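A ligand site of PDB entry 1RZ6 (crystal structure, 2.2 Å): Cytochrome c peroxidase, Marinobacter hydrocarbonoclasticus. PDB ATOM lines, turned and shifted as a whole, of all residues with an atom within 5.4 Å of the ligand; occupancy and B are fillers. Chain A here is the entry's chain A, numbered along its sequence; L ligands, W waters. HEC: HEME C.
O of Phe 38 is in hydrogen-bond range of N of Cys 51. O of Cys 54 sits at hydrogen-bond distance from OG of Ser 80, 3.4 Å away. The backbone carbonyl oxygen (O) of Pro 81 is in hydrogen-bond range of a ring nitrogen (ND1) of His 55. A ring nitrogen (ND1) of His 71 lies within hydrogen-bond range of the backbone carbonyl oxygen of Ala 111 (3.4 Å). A ring nitrogen (ND1) of His 71 is in hydrogen-bond range of the backbone carbonyl oxygen of Glu 114. The guanidinium group (NH1) of Arg 246 sits at hydrogen-bond distance from the side-chain amide oxygen (OD1) of Asn 89 (3.3 Å). N of Ile 69 lies within hydrogen-bond range of OG1 of Thr 67, 3.1 Å away. The backbone NH of Ser 50 sits at hydrogen-bond distance from the side-chain hydroxyl of Thr 53 (2.9 Å).
Water W4 lies within hydrogen-bond range of an oxygen (O1A) of the ligand (2.6 Å), the backbone carbonyl oxygen (O) of Thr 82 (2.7 Å) and the guanidinium group (NH2) of Arg 246 (3.5 Å). Water W5 bridges an oxygen (O2D) of the ligand (2.9 Å) and the backbone carbonyl oxygen of His 71 (3.2 Å). Water W2 lies within hydrogen-bond range of O of Ala 111 (2.8 Å), OE1 of Glu 114 (3.0 Å) and O1D of the ligand (3.1 Å). Water W3 lies within hydrogen-bond range of O of Glu 114 (2.7 Å), O of Gly 112 (3.2 Å) and ND1 of His 71 (3.3 Å). Water W1 lies within hydrogen-bond range of the backbone carbonyl oxygen (O) of Phe 93 (3.2 Å) and an oxygen (O1D) of the ligand (3.5 Å).
A carbon (CAB) of the ligand is covalently linked to the side-chain sulfur (SG) of Cys 51 (1.8 Å). The side-chain sulfur (SG) of Cys 54 is bonded to a carbon (CAC) of the ligand (1.9 Å). A ring nitrogen (NE2) of His 55 binds an iron atom (FE) of the ligand, at 2.0 Å. A ring nitrogen (NE2) of His 71 is bound to an iron atom (FE) of the ligand, 2.2 Å away. An oxygen (O1A) of the ligand lies within salt-bridge range of the guanidinium group of Arg 246 (2.8 Å). The backbone NH (N) of Phe 93 lies within hydrogen-bond range of an oxygen (O2A) of the ligand. NH1 of Arg 78 lies within salt-bridge range of O2D of the ligand. OD1 of Asn 89 sits close to O1A of the ligand (3.4 Å).
Merely in contact with the ligand: Glu 160 (3.1 Å), Gly 112 (3.3 Å), Pro 108 (3.4 Å), Pro 81 (3.4 Å), Gln 92 (3.4 Å), Ile 69 (3.4 Å), Ile 49 (3.4 Å), Ser 50 (3.5 Å), Met 115 (3.5 Å), Ile 156 (3.6 Å), Asn 79 (3.6 Å), Trp 73 (3.7 Å), Ala 86 (3.7 Å), Ser 80 (3.8 Å), Gly 70 (3.8 Å), Val 83 (3.96 Å), Thr 67 (3.99 Å) and Phe 38 (3.99 Å). Hydrophobic or aromatic side chains that line the ligand: Phe 38, Ile 49, His 55, Ile 69, His 71, Trp 73, Pro 81, Val 83, Ala 86, Phe 93, Pro 108, Met 115 and Ile 156. Of the 34 residues printed, 26 come within 4 Å of the ligand.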
ATOM      1  N   PHE A  38     -29.669 -13.837 -20.598  1.00  0.00           N
ATOM      2  CA  PHE A  38     -28.268 -14.075 -20.912  1.00  0.00           C
ATOM      3  C   PHE A  38     -27.546 -14.567 -19.633  1.00  0.00           C
ATOM      4  O   PHE A  38     -26.672 -15.436 -19.695  1.00  0.00           O
ATOM      5  CB  PHE A  38     -27.634 -12.782 -21.435  1.00  0.00           C
ATOM      6  CG  PHE A  38     -26.228 -12.966 -21.958  1.00  0.00           C
ATOM      7  CD1 PHE A  38     -26.008 -13.370 -23.278  1.00  0.00           C
ATOM      8  CD2 PHE A  38     -25.132 -12.766 -21.125  1.00  0.00           C
ATOM      9  CE1 PHE A  38     -24.713 -13.568 -23.759  1.00  0.00           C
ATOM     10  CE2 PHE A  38     -23.833 -12.954 -21.587  1.00  0.00           C
ATOM     11  CZ  PHE A  38     -23.617 -13.358 -22.917  1.00  0.00           C
ATOM     12  N   ILE A  49     -25.288 -23.422 -15.495  1.00  0.00           N
ATOM     13  CA  ILE A  49     -24.752 -22.751 -16.671  1.00  0.00           C
ATOM     14  C   ILE A  49     -25.666 -21.692 -17.314  1.00  0.00           C
ATOM     15  O   ILE A  49     -26.871 -21.889 -17.433  1.00  0.00           O
ATOM     16  CB  ILE A  49     -24.417 -23.817 -17.738  1.00  0.00           C
ATOM     17  CG1 ILE A  49     -23.382 -24.798 -17.188  1.00  0.00           C
ATOM     18  CG2 ILE A  49     -23.914 -23.164 -19.008  1.00  0.00           C
ATOM     19  CD1 ILE A  49     -23.144 -26.020 -18.090  1.00  0.00           C
ATOM     20  N   SER A  50     -25.078 -20.563 -17.711  1.00  0.00           N
ATOM     21  CA  SER A  50     -25.826 -19.508 -18.382  1.00  0.00           C
ATOM     22  C   SER A  50     -24.962 -19.081 -19.586  1.00  0.00           C
ATOM     23  O   SER A  50     -23.850 -19.569 -19.743  1.00  0.00           O
ATOM     24  CB  SER A  50     -26.052 -18.303 -17.462  1.00  0.00           C
ATOM     25  OG  SER A  50     -24.873 -17.527 -17.355  1.00  0.00           O
ATOM     26  N   CYS A  51     -25.474 -18.197 -20.426  1.00  0.00           N
ATOM     27  CA  CYS A  51     -24.699 -17.739 -21.589  1.00  0.00           C
ATOM     28  C   CYS A  51     -23.385 -17.109 -21.104  1.00  0.00           C
ATOM     29  O   CYS A  51     -22.323 -17.329 -21.690  1.00  0.00           O
ATOM     30  CB  CYS A  51     -25.467 -16.656 -22.382  1.00  0.00           C
ATOM     31  SG  CYS A  51     -27.169 -17.035 -22.819  1.00  0.00           S
ATOM     32  N   THR A  53     -21.602 -17.821 -18.703  1.00  0.00           N
ATOM     33  CA  THR A  53     -20.639 -18.827 -18.328  1.00  0.00           C
ATOM     34  C   THR A  53     -19.646 -19.048 -19.465  1.00  0.00           C
ATOM     35  O   THR A  53     -18.445 -19.129 -19.237  1.00  0.00           O
ATOM     36  CB  THR A  53     -21.331 -20.162 -18.037  1.00  0.00           C
ATOM     37  OG1 THR A  53     -22.302 -19.966 -17.002  1.00  0.00           O
ATOM     38  CG2 THR A  53     -20.302 -21.205 -17.598  1.00  0.00           C
ATOM     39  N   CYS A  54     -20.123 -19.137 -20.704  1.00  0.00           N
ATOM     40  CA  CYS A  54     -19.209 -19.366 -21.822  1.00  0.00           C
ATOM     41  C   CYS A  54     -18.876 -18.139 -22.657  1.00  0.00           C
ATOM     42  O   CYS A  54     -17.973 -18.167 -23.488  1.00  0.00           O
ATOM     43  CB  CYS A  54     -19.754 -20.467 -22.724  1.00  0.00           C
ATOM     44  SG  CYS A  54     -20.043 -22.074 -21.887  1.00  0.00           S
ATOM     45  N   HIS A  55     -19.613 -17.055 -22.426  1.00  0.00           N
ATOM     46  CA  HIS A  55     -19.401 -15.814 -23.165  1.00  0.00           C
ATOM     47  C   HIS A  55     -19.366 -14.706 -22.108  1.00  0.00           C
ATOM     48  O   HIS A  55     -20.219 -13.821 -22.066  1.00  0.00           O
ATOM     49  CB  HIS A  55     -20.565 -15.588 -24.154  1.00  0.00           C
ATOM     50  CG  HIS A  55     -20.739 -16.697 -25.148  1.00  0.00           C
ATOM     51  ND1 HIS A  55     -19.873 -16.916 -26.186  1.00  0.00           N
ATOM     52  CD2 HIS A  55     -21.703 -17.650 -25.256  1.00  0.00           C
ATOM     53  CE1 HIS A  55     -20.302 -17.941 -26.912  1.00  0.00           C
ATOM     54  NE2 HIS A  55     -21.409 -18.408 -26.363  1.00  0.00           N
ATOM     55  N   ASP A  63     -15.001 -17.981 -23.791  1.00  0.00           N
ATOM     56  CA  ASP A  63     -14.613 -18.966 -22.790  1.00  0.00           C
ATOM     57  C   ASP A  63     -13.114 -19.213 -22.883  1.00  0.00           C
ATOM     58  O   ASP A  63     -12.546 -19.254 -23.964  1.00  0.00           O
ATOM     59  CB  ASP A  63     -15.330 -20.283 -23.068  1.00  0.00           C
ATOM     60  CG  ASP A  63     -15.418 -21.191 -21.866  1.00  0.00           C
ATOM     61  OD1 ASP A  63     -14.498 -21.164 -21.021  1.00  0.00           O
ATOM     62  OD2 ASP A  63     -16.406 -21.946 -21.778  1.00  0.00           O
ATOM     63  N   THR A  67     -14.821 -26.348 -24.864  1.00  0.00           N
ATOM     64  CA  THR A  67     -15.918 -27.110 -24.265  1.00  0.00           C
ATOM     65  C   THR A  67     -16.637 -27.992 -25.290  1.00  0.00           C
ATOM     66  O   THR A  67     -16.589 -27.728 -26.492  1.00  0.00           O
ATOM     67  CB  THR A  67     -16.941 -26.154 -23.600  1.00  0.00           C
ATOM     68  OG1 THR A  67     -18.039 -26.916 -23.086  1.00  0.00           O
ATOM     69  CG2 THR A  67     -17.466 -25.139 -24.595  1.00  0.00           C
ATOM     70  N   ILE A  69     -19.938 -28.839 -24.635  1.00  0.00           N
ATOM     71  CA  ILE A  69     -21.362 -28.606 -24.441  1.00  0.00           C
ATOM     72  C   ILE A  69     -21.806 -27.227 -24.928  1.00  0.00           C
ATOM     73  O   ILE A  69     -21.002 -26.418 -25.380  1.00  0.00           O
ATOM     74  CB  ILE A  69     -21.758 -28.806 -22.967  1.00  0.00           C
ATOM     75  CG1 ILE A  69     -20.931 -27.888 -22.069  1.00  0.00           C
ATOM     76  CG2 ILE A  69     -21.515 -30.271 -22.571  1.00  0.00           C
ATOM     77  CD1 ILE A  69     -21.497 -27.767 -20.675  1.00  0.00           C
ATOM     78  N   GLY A  70     -23.112 -26.987 -24.851  1.00  0.00           N
ATOM     79  CA  GLY A  70     -23.688 -25.740 -25.301  1.00  0.00           C
ATOM     80  C   GLY A  70     -24.246 -25.898 -26.708  1.00  0.00           C
ATOM     81  O   GLY A  70     -23.662 -26.602 -27.541  1.00  0.00           O
ATOM     82  N   HIS A  71     -25.374 -25.237 -26.974  1.00  0.00           N
ATOM     83  CA  HIS A  71     -26.022 -25.271 -28.283  1.00  0.00           C
ATOM     84  C   HIS A  71     -26.319 -26.677 -28.803  1.00  0.00           C
ATOM     85  O   HIS A  71     -26.240 -26.939 -30.008  1.00  0.00           O
ATOM     86  CB  HIS A  71     -25.155 -24.518 -29.288  1.00  0.00           C
ATOM     87  CG  HIS A  71     -24.831 -23.126 -28.850  1.00  0.00           C
ATOM     88  ND1 HIS A  71     -25.811 -22.168 -28.671  1.00  0.00           N
ATOM     89  CD2 HIS A  71     -23.667 -22.549 -28.499  1.00  0.00           C
ATOM     90  CE1 HIS A  71     -25.260 -21.053 -28.231  1.00  0.00           C
ATOM     91  NE2 HIS A  71     -23.954 -21.263 -28.118  1.00  0.00           N
ATOM     92  N   TRP A  73     -24.616 -29.258 -28.740  1.00  0.00           N
ATOM     93  CA  TRP A  73     -23.464 -29.836 -29.417  1.00  0.00           C
ATOM     94  C   TRP A  73     -23.263 -31.300 -29.017  1.00  0.00           C
ATOM     95  O   TRP A  73     -23.355 -31.645 -27.835  1.00  0.00           O
ATOM     96  CB  TRP A  73     -22.224 -29.006 -29.092  1.00  0.00           C
ATOM     97  CG  TRP A  73     -20.970 -29.397 -29.820  1.00  0.00           C
ATOM     98  CD1 TRP A  73     -20.093 -30.382 -29.458  1.00  0.00           C
ATOM     99  CD2 TRP A  73     -20.419 -28.765 -30.978  1.00  0.00           C
ATOM    100  NE1 TRP A  73     -19.021 -30.392 -30.320  1.00  0.00           N
ATOM    101  CE2 TRP A  73     -19.199 -29.422 -31.269  1.00  0.00           C
ATOM    102  CE3 TRP A  73     -20.837 -27.706 -31.813  1.00  0.00           C
ATOM    103  CZ2 TRP A  73     -18.373 -29.046 -32.347  1.00  0.00           C
ATOM    104  CZ3 TRP A  73     -20.020 -27.332 -32.888  1.00  0.00           C
ATOM    105  CH2 TRP A  73     -18.804 -28.010 -33.144  1.00  0.00           C
ATOM    106  N   ARG A  78     -14.613 -27.622 -28.527  1.00  0.00           N
ATOM    107  CA  ARG A  78     -14.235 -26.588 -29.470  1.00  0.00           C
ATOM    108  C   ARG A  78     -14.155 -25.273 -28.714  1.00  0.00           C
ATOM    109  O   ARG A  78     -14.751 -25.127 -27.641  1.00  0.00           O
ATOM    110  CB  ARG A  78     -15.256 -26.493 -30.620  1.00  0.00           C
ATOM    111  CG  ARG A  78     -16.511 -25.689 -30.306  1.00  0.00           C
ATOM    112  CD  ARG A  78     -17.772 -26.536 -30.324  1.00  0.00           C
ATOM    113  NE  ARG A  78     -18.131 -27.013 -29.003  1.00  0.00           N
ATOM    114  CZ  ARG A  78     -19.326 -26.834 -28.418  1.00  0.00           C
ATOM    115  NH1 ARG A  78     -20.303 -26.199 -29.048  1.00  0.00           N
ATOM    116  NH2 ARG A  78     -19.520 -27.285 -27.192  1.00  0.00           N
ATOM    117  N   ASN A  79     -13.412 -24.325 -29.272  1.00  0.00           N
ATOM    118  CA  ASN A  79     -13.226 -23.016 -28.671  1.00  0.00           C
ATOM    119  C   ASN A  79     -14.520 -22.219 -28.834  1.00  0.00           C
ATOM    120  O   ASN A  79     -15.283 -22.456 -29.764  1.00  0.00           O
ATOM    121  CB  ASN A  79     -12.083 -22.294 -29.401  1.00  0.00           C
ATOM    122  CG  ASN A  79     -11.622 -21.047 -28.693  1.00  0.00           C
ATOM    123  OD1 ASN A  79     -10.912 -20.218 -29.262  1.00  0.00           O
ATOM    124  ND2 ASN A  79     -12.003 -20.904 -27.432  1.00  0.00           N
ATOM    125  N   SER A  80     -14.769 -21.276 -27.928  1.00  0.00           N
ATOM    126  CA  SER A  80     -15.975 -20.479 -28.059  1.00  0.00           C
ATOM    127  C   SER A  80     -15.618 -19.094 -28.594  1.00  0.00           C
ATOM    128  O   SER A  80     -14.637 -18.478 -28.157  1.00  0.00           O
ATOM    129  CB  SER A  80     -16.679 -20.338 -26.701  1.00  0.00           C
ATOM    130  OG  SER A  80     -15.936 -19.500 -25.841  1.00  0.00           O
ATOM    131  N   PRO A  81     -16.390 -18.606 -29.576  1.00  0.00           N
ATOM    132  CA  PRO A  81     -16.168 -17.292 -30.163  1.00  0.00           C
ATOM    133  C   PRO A  81     -16.709 -16.251 -29.190  1.00  0.00           C
ATOM    134  O   PRO A  81     -17.432 -16.603 -28.258  1.00  0.00           O
ATOM    135  CB  PRO A  81     -17.008 -17.349 -31.442  1.00  0.00           C
ATOM    136  CG  PRO A  81     -18.210 -18.155 -30.972  1.00  0.00           C
ATOM    137  CD  PRO A  81     -17.556 -19.263 -30.178  1.00  0.00           C
ATOM    138  N   THR A  82     -16.355 -14.991 -29.405  1.00  0.00           N
ATOM    139  CA  THR A  82     -16.841 -13.937 -28.538  1.00  0.00           C
ATOM    140  C   THR A  82     -18.217 -13.464 -29.020  1.00  0.00           C
ATOM    141  O   THR A  82     -18.498 -13.479 -30.219  1.00  0.00           O
ATOM    142  CB  THR A  82     -15.923 -12.696 -28.553  1.00  0.00           C
ATOM    143  OG1 THR A  82     -16.511 -11.665 -27.765  1.00  0.00           O
ATOM    144  CG2 THR A  82     -15.719 -12.170 -29.992  1.00  0.00           C
ATOM    145  N   VAL A  83     -19.067 -13.045 -28.079  1.00  0.00           N
ATOM    146  CA  VAL A  83     -20.368 -12.525 -28.453  1.00  0.00           C
ATOM    147  C   VAL A  83     -20.216 -11.064 -28.876  1.00  0.00           C
ATOM    148  O   VAL A  83     -21.098 -10.509 -29.535  1.00  0.00           O
ATOM    149  CB  VAL A  83     -21.386 -12.596 -27.295  1.00  0.00           C
ATOM    150  CG1 VAL A  83     -21.817 -14.037 -27.070  1.00  0.00           C
ATOM    151  CG2 VAL A  83     -20.784 -11.987 -26.024  1.00  0.00           C
ATOM    152  N   ALA A  86     -20.719  -9.873 -32.594  1.00  0.00           N
ATOM    153  CA  ALA A  86     -21.095 -11.049 -33.382  1.00  0.00           C
ATOM    154  C   ALA A  86     -22.224 -10.702 -34.350  1.00  0.00           C
ATOM    155  O   ALA A  86     -22.325 -11.271 -35.434  1.00  0.00           O
ATOM    156  CB  ALA A  86     -21.505 -12.202 -32.449  1.00  0.00           C
ATOM    157  N   ASN A  89     -21.379 -10.275 -38.002  1.00  0.00           N
ATOM    158  CA  ASN A  89     -20.847 -11.381 -38.807  1.00  0.00           C
ATOM    159  C   ASN A  89     -21.969 -12.058 -39.594  1.00  0.00           C
ATOM    160  O   ASN A  89     -22.997 -12.415 -39.030  1.00  0.00           O
ATOM    161  CB  ASN A  89     -20.167 -12.423 -37.909  1.00  0.00           C
ATOM    162  CG  ASN A  89     -19.024 -11.844 -37.070  1.00  0.00           C
ATOM    163  OD1 ASN A  89     -18.873 -12.186 -35.882  1.00  0.00           O
ATOM    164  ND2 ASN A  89     -18.209 -10.991 -37.668  1.00  0.00           N
ATOM    165  N   ALA A  91     -21.370 -14.854 -41.394  1.00  0.00           N
ATOM    166  CA  ALA A  91     -21.083 -16.277 -41.199  1.00  0.00           C
ATOM    167  C   ALA A  91     -21.004 -16.535 -39.692  1.00  0.00           C
ATOM    168  O   ALA A  91     -20.749 -15.621 -38.916  1.00  0.00           O
ATOM    169  CB  ALA A  91     -19.740 -16.648 -41.855  1.00  0.00           C
ATOM    170  N   GLN A  92     -21.232 -17.777 -39.279  1.00  0.00           N
ATOM    171  CA  GLN A  92     -21.137 -18.093 -37.848  1.00  0.00           C
ATOM    172  C   GLN A  92     -19.901 -18.954 -37.617  1.00  0.00           C
ATOM    173  O   GLN A  92     -19.299 -19.480 -38.555  1.00  0.00           O
ATOM    174  CB  GLN A  92     -22.378 -18.855 -37.367  1.00  0.00           C
ATOM    175  CG  GLN A  92     -22.557 -20.234 -38.019  1.00  0.00           C
ATOM    176  CD  GLN A  92     -23.374 -21.191 -37.177  1.00  0.00           C
ATOM    177  OE1 GLN A  92     -22.889 -21.744 -36.181  1.00  0.00           O
ATOM    178  NE2 GLN A  92     -24.637 -21.379 -37.554  1.00  0.00           N
ATOM    179  N   PHE A  93     -19.524 -19.093 -36.346  1.00  0.00           N
ATOM    180  CA  PHE A  93     -18.392 -19.928 -35.971  1.00  0.00           C
ATOM    181  C   PHE A  93     -18.698 -21.294 -36.577  1.00  0.00           C
ATOM    182  O   PHE A  93     -19.824 -21.793 -36.468  1.00  0.00           O
ATOM    183  CB  PHE A  93     -18.322 -20.055 -34.438  1.00  0.00           C
ATOM    184  CG  PHE A  93     -17.351 -21.090 -33.947  1.00  0.00           C
ATOM    185  CD1 PHE A  93     -16.133 -20.718 -33.375  1.00  0.00           C
ATOM    186  CD2 PHE A  93     -17.656 -22.449 -34.031  1.00  0.00           C
ATOM    187  CE1 PHE A  93     -15.225 -21.676 -32.888  1.00  0.00           C
ATOM    188  CE2 PHE A  93     -16.759 -23.419 -33.549  1.00  0.00           C
ATOM    189  CZ  PHE A  93     -15.541 -23.027 -32.968  1.00  0.00           C
ATOM    190  N   PRO A 108     -24.944 -15.695 -36.539  1.00  0.00           N
ATOM    191  CA  PRO A 108     -24.401 -15.776 -35.173  1.00  0.00           C
ATOM    192  C   PRO A 108     -25.464 -15.560 -34.106  1.00  0.00           C
ATOM    193  O   PRO A 108     -25.634 -16.372 -33.203  1.00  0.00           O
ATOM    194  CB  PRO A 108     -23.364 -14.642 -35.138  1.00  0.00           C
ATOM    195  CG  PRO A 108     -22.911 -14.553 -36.560  1.00  0.00           C
ATOM    196  CD  PRO A 108     -24.193 -14.722 -37.348  1.00  0.00           C
ATOM    197  N   VAL A 109     -26.182 -14.449 -34.237  1.00  0.00           N
ATOM    198  CA  VAL A 109     -27.233 -14.075 -33.304  1.00  0.00           C
ATOM    199  C   VAL A 109     -28.246 -15.215 -33.166  1.00  0.00           C
ATOM    200  O   VAL A 109     -28.662 -15.561 -32.058  1.00  0.00           O
ATOM    201  CB  VAL A 109     -27.907 -12.768 -33.775  1.00  0.00           C
ATOM    202  CG1 VAL A 109     -29.302 -12.623 -33.190  1.00  0.00           C
ATOM    203  CG2 VAL A 109     -27.036 -11.581 -33.373  1.00  0.00           C
ATOM    204  N   ALA A 111     -27.621 -18.472 -34.172  1.00  0.00           N
ATOM    205  CA  ALA A 111     -26.938 -19.674 -33.701  1.00  0.00           C
ATOM    206  C   ALA A 111     -26.852 -19.603 -32.179  1.00  0.00           C
ATOM    207  O   ALA A 111     -26.890 -20.620 -31.479  1.00  0.00           O
ATOM    208  CB  ALA A 111     -25.543 -19.747 -34.303  1.00  0.00           C
ATOM    209  N   GLY A 112     -26.762 -18.376 -31.676  1.00  0.00           N
ATOM    210  CA  GLY A 112     -26.672 -18.149 -30.252  1.00  0.00           C
ATOM    211  C   GLY A 112     -27.834 -18.671 -29.423  1.00  0.00           C
ATOM    212  O   GLY A 112     -27.661 -18.968 -28.236  1.00  0.00           O
ATOM    213  N   VAL A 113     -29.014 -18.788 -30.028  1.00  0.00           N
ATOM    214  CA  VAL A 113     -30.167 -19.267 -29.292  1.00  0.00           C
ATOM    215  C   VAL A 113     -30.501 -20.734 -29.517  1.00  0.00           C
ATOM    216  O   VAL A 113     -31.569 -21.211 -29.131  1.00  0.00           O
ATOM    217  CB  VAL A 113     -31.406 -18.364 -29.536  1.00  0.00           C
ATOM    218  CG1 VAL A 113     -31.133 -16.985 -28.951  1.00  0.00           C
ATOM    219  CG2 VAL A 113     -31.733 -18.254 -31.037  1.00  0.00           C
ATOM    220  N   GLU A 114     -29.584 -21.457 -30.150  1.00  0.00           N
ATOM    221  CA  GLU A 114     -29.756 -22.888 -30.331  1.00  0.00           C
ATOM    222  C   GLU A 114     -29.467 -23.406 -28.913  1.00  0.00           C
ATOM    223  O   GLU A 114     -28.387 -23.126 -28.358  1.00  0.00           O
ATOM    224  CB  GLU A 114     -28.719 -23.439 -31.320  1.00  0.00           C
ATOM    225  CG  GLU A 114     -29.004 -23.064 -32.782  1.00  0.00           C
ATOM    226  CD  GLU A 114     -27.820 -23.305 -33.721  1.00  0.00           C
ATOM    227  OE1 GLU A 114     -26.888 -24.062 -33.364  1.00  0.00           O
ATOM    228  OE2 GLU A 114     -27.840 -22.739 -34.835  1.00  0.00           O
ATOM    229  N   MET A 115     -30.393 -24.150 -28.314  1.00  0.00           N
ATOM    230  CA  MET A 115     -30.177 -24.643 -26.957  1.00  0.00           C
ATOM    231  C   MET A 115     -30.143 -26.153 -26.790  1.00  0.00           C
ATOM    232  O   MET A 115     -30.665 -26.900 -27.621  1.00  0.00           O
ATOM    233  CB  MET A 115     -31.253 -24.070 -26.029  1.00  0.00           C
ATOM    234  CG  MET A 115     -31.223 -22.557 -25.942  1.00  0.00           C
ATOM    235  SD  MET A 115     -32.308 -21.958 -24.650  1.00  0.00           S
ATOM    236  CE  MET A 115     -31.632 -20.332 -24.381  1.00  0.00           C
ATOM    237  N   ILE A 156     -33.428 -12.627 -26.285  1.00  0.00           N
ATOM    238  CA  ILE A 156     -31.984 -12.857 -26.166  1.00  0.00           C
ATOM    239  C   ILE A 156     -31.258 -12.246 -27.365  1.00  0.00           C
ATOM    240  O   ILE A 156     -30.216 -11.604 -27.209  1.00  0.00           O
ATOM    241  CB  ILE A 156     -31.673 -14.367 -26.048  1.00  0.00           C
ATOM    242  CG1 ILE A 156     -32.238 -14.911 -24.732  1.00  0.00           C
ATOM    243  CG2 ILE A 156     -30.174 -14.604 -26.131  1.00  0.00           C
ATOM    244  CD1 ILE A 156     -32.172 -16.393 -24.579  1.00  0.00           C
ATOM    245  N   GLU A 160     -28.204  -9.614 -27.553  1.00  0.00           N
ATOM    246  CA  GLU A 160     -26.974  -9.938 -28.278  1.00  0.00           C
ATOM    247  C   GLU A 160     -26.560  -8.805 -29.211  1.00  0.00           C
ATOM    248  O   GLU A 160     -25.379  -8.498 -29.347  1.00  0.00           O
ATOM    249  CB  GLU A 160     -27.142 -11.221 -29.101  1.00  0.00           C
ATOM    250  CG  GLU A 160     -27.220 -12.504 -28.292  1.00  0.00           C
ATOM    251  CD  GLU A 160     -27.396 -13.727 -29.159  1.00  0.00           C
ATOM    252  OE1 GLU A 160     -26.451 -14.529 -29.253  1.00  0.00           O
ATOM    253  OE2 GLU A 160     -28.485 -13.886 -29.752  1.00  0.00           O
ATOM    254  N   ARG A 246     -14.741 -20.559 -40.240  1.00  0.00           N
ATOM    255  CA  ARG A 246     -15.054 -19.172 -40.551  1.00  0.00           C
ATOM    256  C   ARG A 246     -13.765 -18.382 -40.347  1.00  0.00           C
ATOM    257  O   ARG A 246     -13.046 -18.606 -39.376  1.00  0.00           O
ATOM    258  CB  ARG A 246     -16.115 -18.606 -39.586  1.00  0.00           C
ATOM    259  CG  ARG A 246     -16.490 -17.162 -39.911  1.00  0.00           C
ATOM    260  CD  ARG A 246     -17.552 -16.606 -38.955  1.00  0.00           C
ATOM    261  NE  ARG A 246     -17.070 -16.588 -37.574  1.00  0.00           N
ATOM    262  CZ  ARG A 246     -17.701 -16.008 -36.565  1.00  0.00           C
ATOM    263  NH1 ARG A 246     -18.853 -15.374 -36.768  1.00  0.00           N
ATOM    264  NH2 ARG A 246     -17.179 -16.093 -35.341  1.00  0.00           N
HETATM  265 FE   HEC L   1     -22.650 -19.726 -27.207  1.00  0.00          FE
HETATM  266  CHA HEC L   1     -21.261 -19.786 -30.242  1.00  0.00           C
HETATM  267  CHB HEC L   1     -24.363 -16.928 -27.967  1.00  0.00           C
HETATM  268  CHC HEC L   1     -24.630 -20.176 -24.504  1.00  0.00           C
HETATM  269  CHD HEC L   1     -20.532 -22.117 -26.125  1.00  0.00           C
HETATM  270  NA  HEC L   1     -22.745 -18.518 -28.823  1.00  0.00           N
HETATM  271  C1A HEC L   1     -22.090 -18.712 -29.999  1.00  0.00           C
HETATM  272  C2A HEC L   1     -22.404 -17.568 -30.857  1.00  0.00           C
HETATM  273  C3A HEC L   1     -23.196 -16.705 -30.184  1.00  0.00           C
HETATM  274  C4A HEC L   1     -23.481 -17.360 -28.919  1.00  0.00           C
HETATM  275  CMA HEC L   1     -23.743 -15.338 -30.632  1.00  0.00           C
HETATM  276  CAA HEC L   1     -21.838 -17.412 -32.283  1.00  0.00           C
HETATM  277  CBA HEC L   1     -20.834 -16.264 -32.471  1.00  0.00           C
HETATM  278  CGA HEC L   1     -20.355 -16.107 -33.898  1.00  0.00           C
HETATM  279  O1A HEC L   1     -19.741 -15.025 -34.141  1.00  0.00           O
HETATM  280  O2A HEC L   1     -20.506 -17.017 -34.713  1.00  0.00           O
HETATM  281  NB  HEC L   1     -24.225 -18.772 -26.414  1.00  0.00           N
HETATM  282  C1B HEC L   1     -24.807 -17.598 -26.867  1.00  0.00           C
HETATM  283  C2B HEC L   1     -25.929 -17.178 -26.060  1.00  0.00           C
HETATM  284  C3B HEC L   1     -26.064 -18.157 -25.136  1.00  0.00           C
HETATM  285  C4B HEC L   1     -24.988 -19.093 -25.309  1.00  0.00           C
HETATM  286  CMB HEC L   1     -26.784 -15.913 -26.259  1.00  0.00           C
HETATM  287  CAB HEC L   1     -27.143 -18.282 -24.058  1.00  0.00           C
HETATM  288  CBB HEC L   1     -28.569 -18.557 -24.625  1.00  0.00           C
HETATM  289  NC  HEC L   1     -22.572 -20.917 -25.597  1.00  0.00           N
HETATM  290  C1C HEC L   1     -23.488 -20.944 -24.576  1.00  0.00           C
HETATM  291  C2C HEC L   1     -22.975 -21.830 -23.533  1.00  0.00           C
HETATM  292  C3C HEC L   1     -21.788 -22.330 -23.930  1.00  0.00           C
HETATM  293  C4C HEC L   1     -21.546 -21.776 -25.256  1.00  0.00           C
HETATM  294  CMC HEC L   1     -23.759 -22.014 -22.206  1.00  0.00           C
HETATM  295  CAC HEC L   1     -20.761 -23.231 -23.212  1.00  0.00           C
HETATM  296  CBC HEC L   1     -21.214 -24.546 -22.572  1.00  0.00           C
HETATM  297  ND  HEC L   1     -21.188 -20.767 -28.006  1.00  0.00           N
HETATM  298  C1D HEC L   1     -20.364 -21.743 -27.433  1.00  0.00           C
HETATM  299  C2D HEC L   1     -19.422 -22.295 -28.387  1.00  0.00           C
HETATM  300  C3D HEC L   1     -19.768 -21.720 -29.575  1.00  0.00           C
HETATM  301  C4D HEC L   1     -20.770 -20.706 -29.306  1.00  0.00           C
HETATM  302  CMD HEC L   1     -18.370 -23.404 -28.069  1.00  0.00           C
HETATM  303  CAD HEC L   1     -19.376 -22.115 -31.012  1.00  0.00           C
HETATM  304  CBD HEC L   1     -19.982 -23.531 -31.174  1.00  0.00           C
HETATM  305  CGD HEC L   1     -21.316 -23.529 -31.881  1.00  0.00           C
HETATM  306  O1D HEC L   1     -21.708 -22.516 -32.476  1.00  0.00           O
HETATM  307  O2D HEC L   1     -22.096 -24.312 -31.322  1.00  0.00           O
HETATM  308  O   HOH W   1     -20.655 -24.581 -35.086  1.00  0.00           O
HETATM  309  O   HOH W   2     -24.757 -22.351 -32.193  1.00  0.00           O
HETATM  310  O   HOH W   3     -28.021 -21.437 -26.294  1.00  0.00           O
HETATM  311  O   HOH W   4     -17.866 -13.782 -32.830  1.00  0.00           O
HETATM  312  O   HOH W   5     -23.961 -26.426 -32.153  1.00  0.00           O
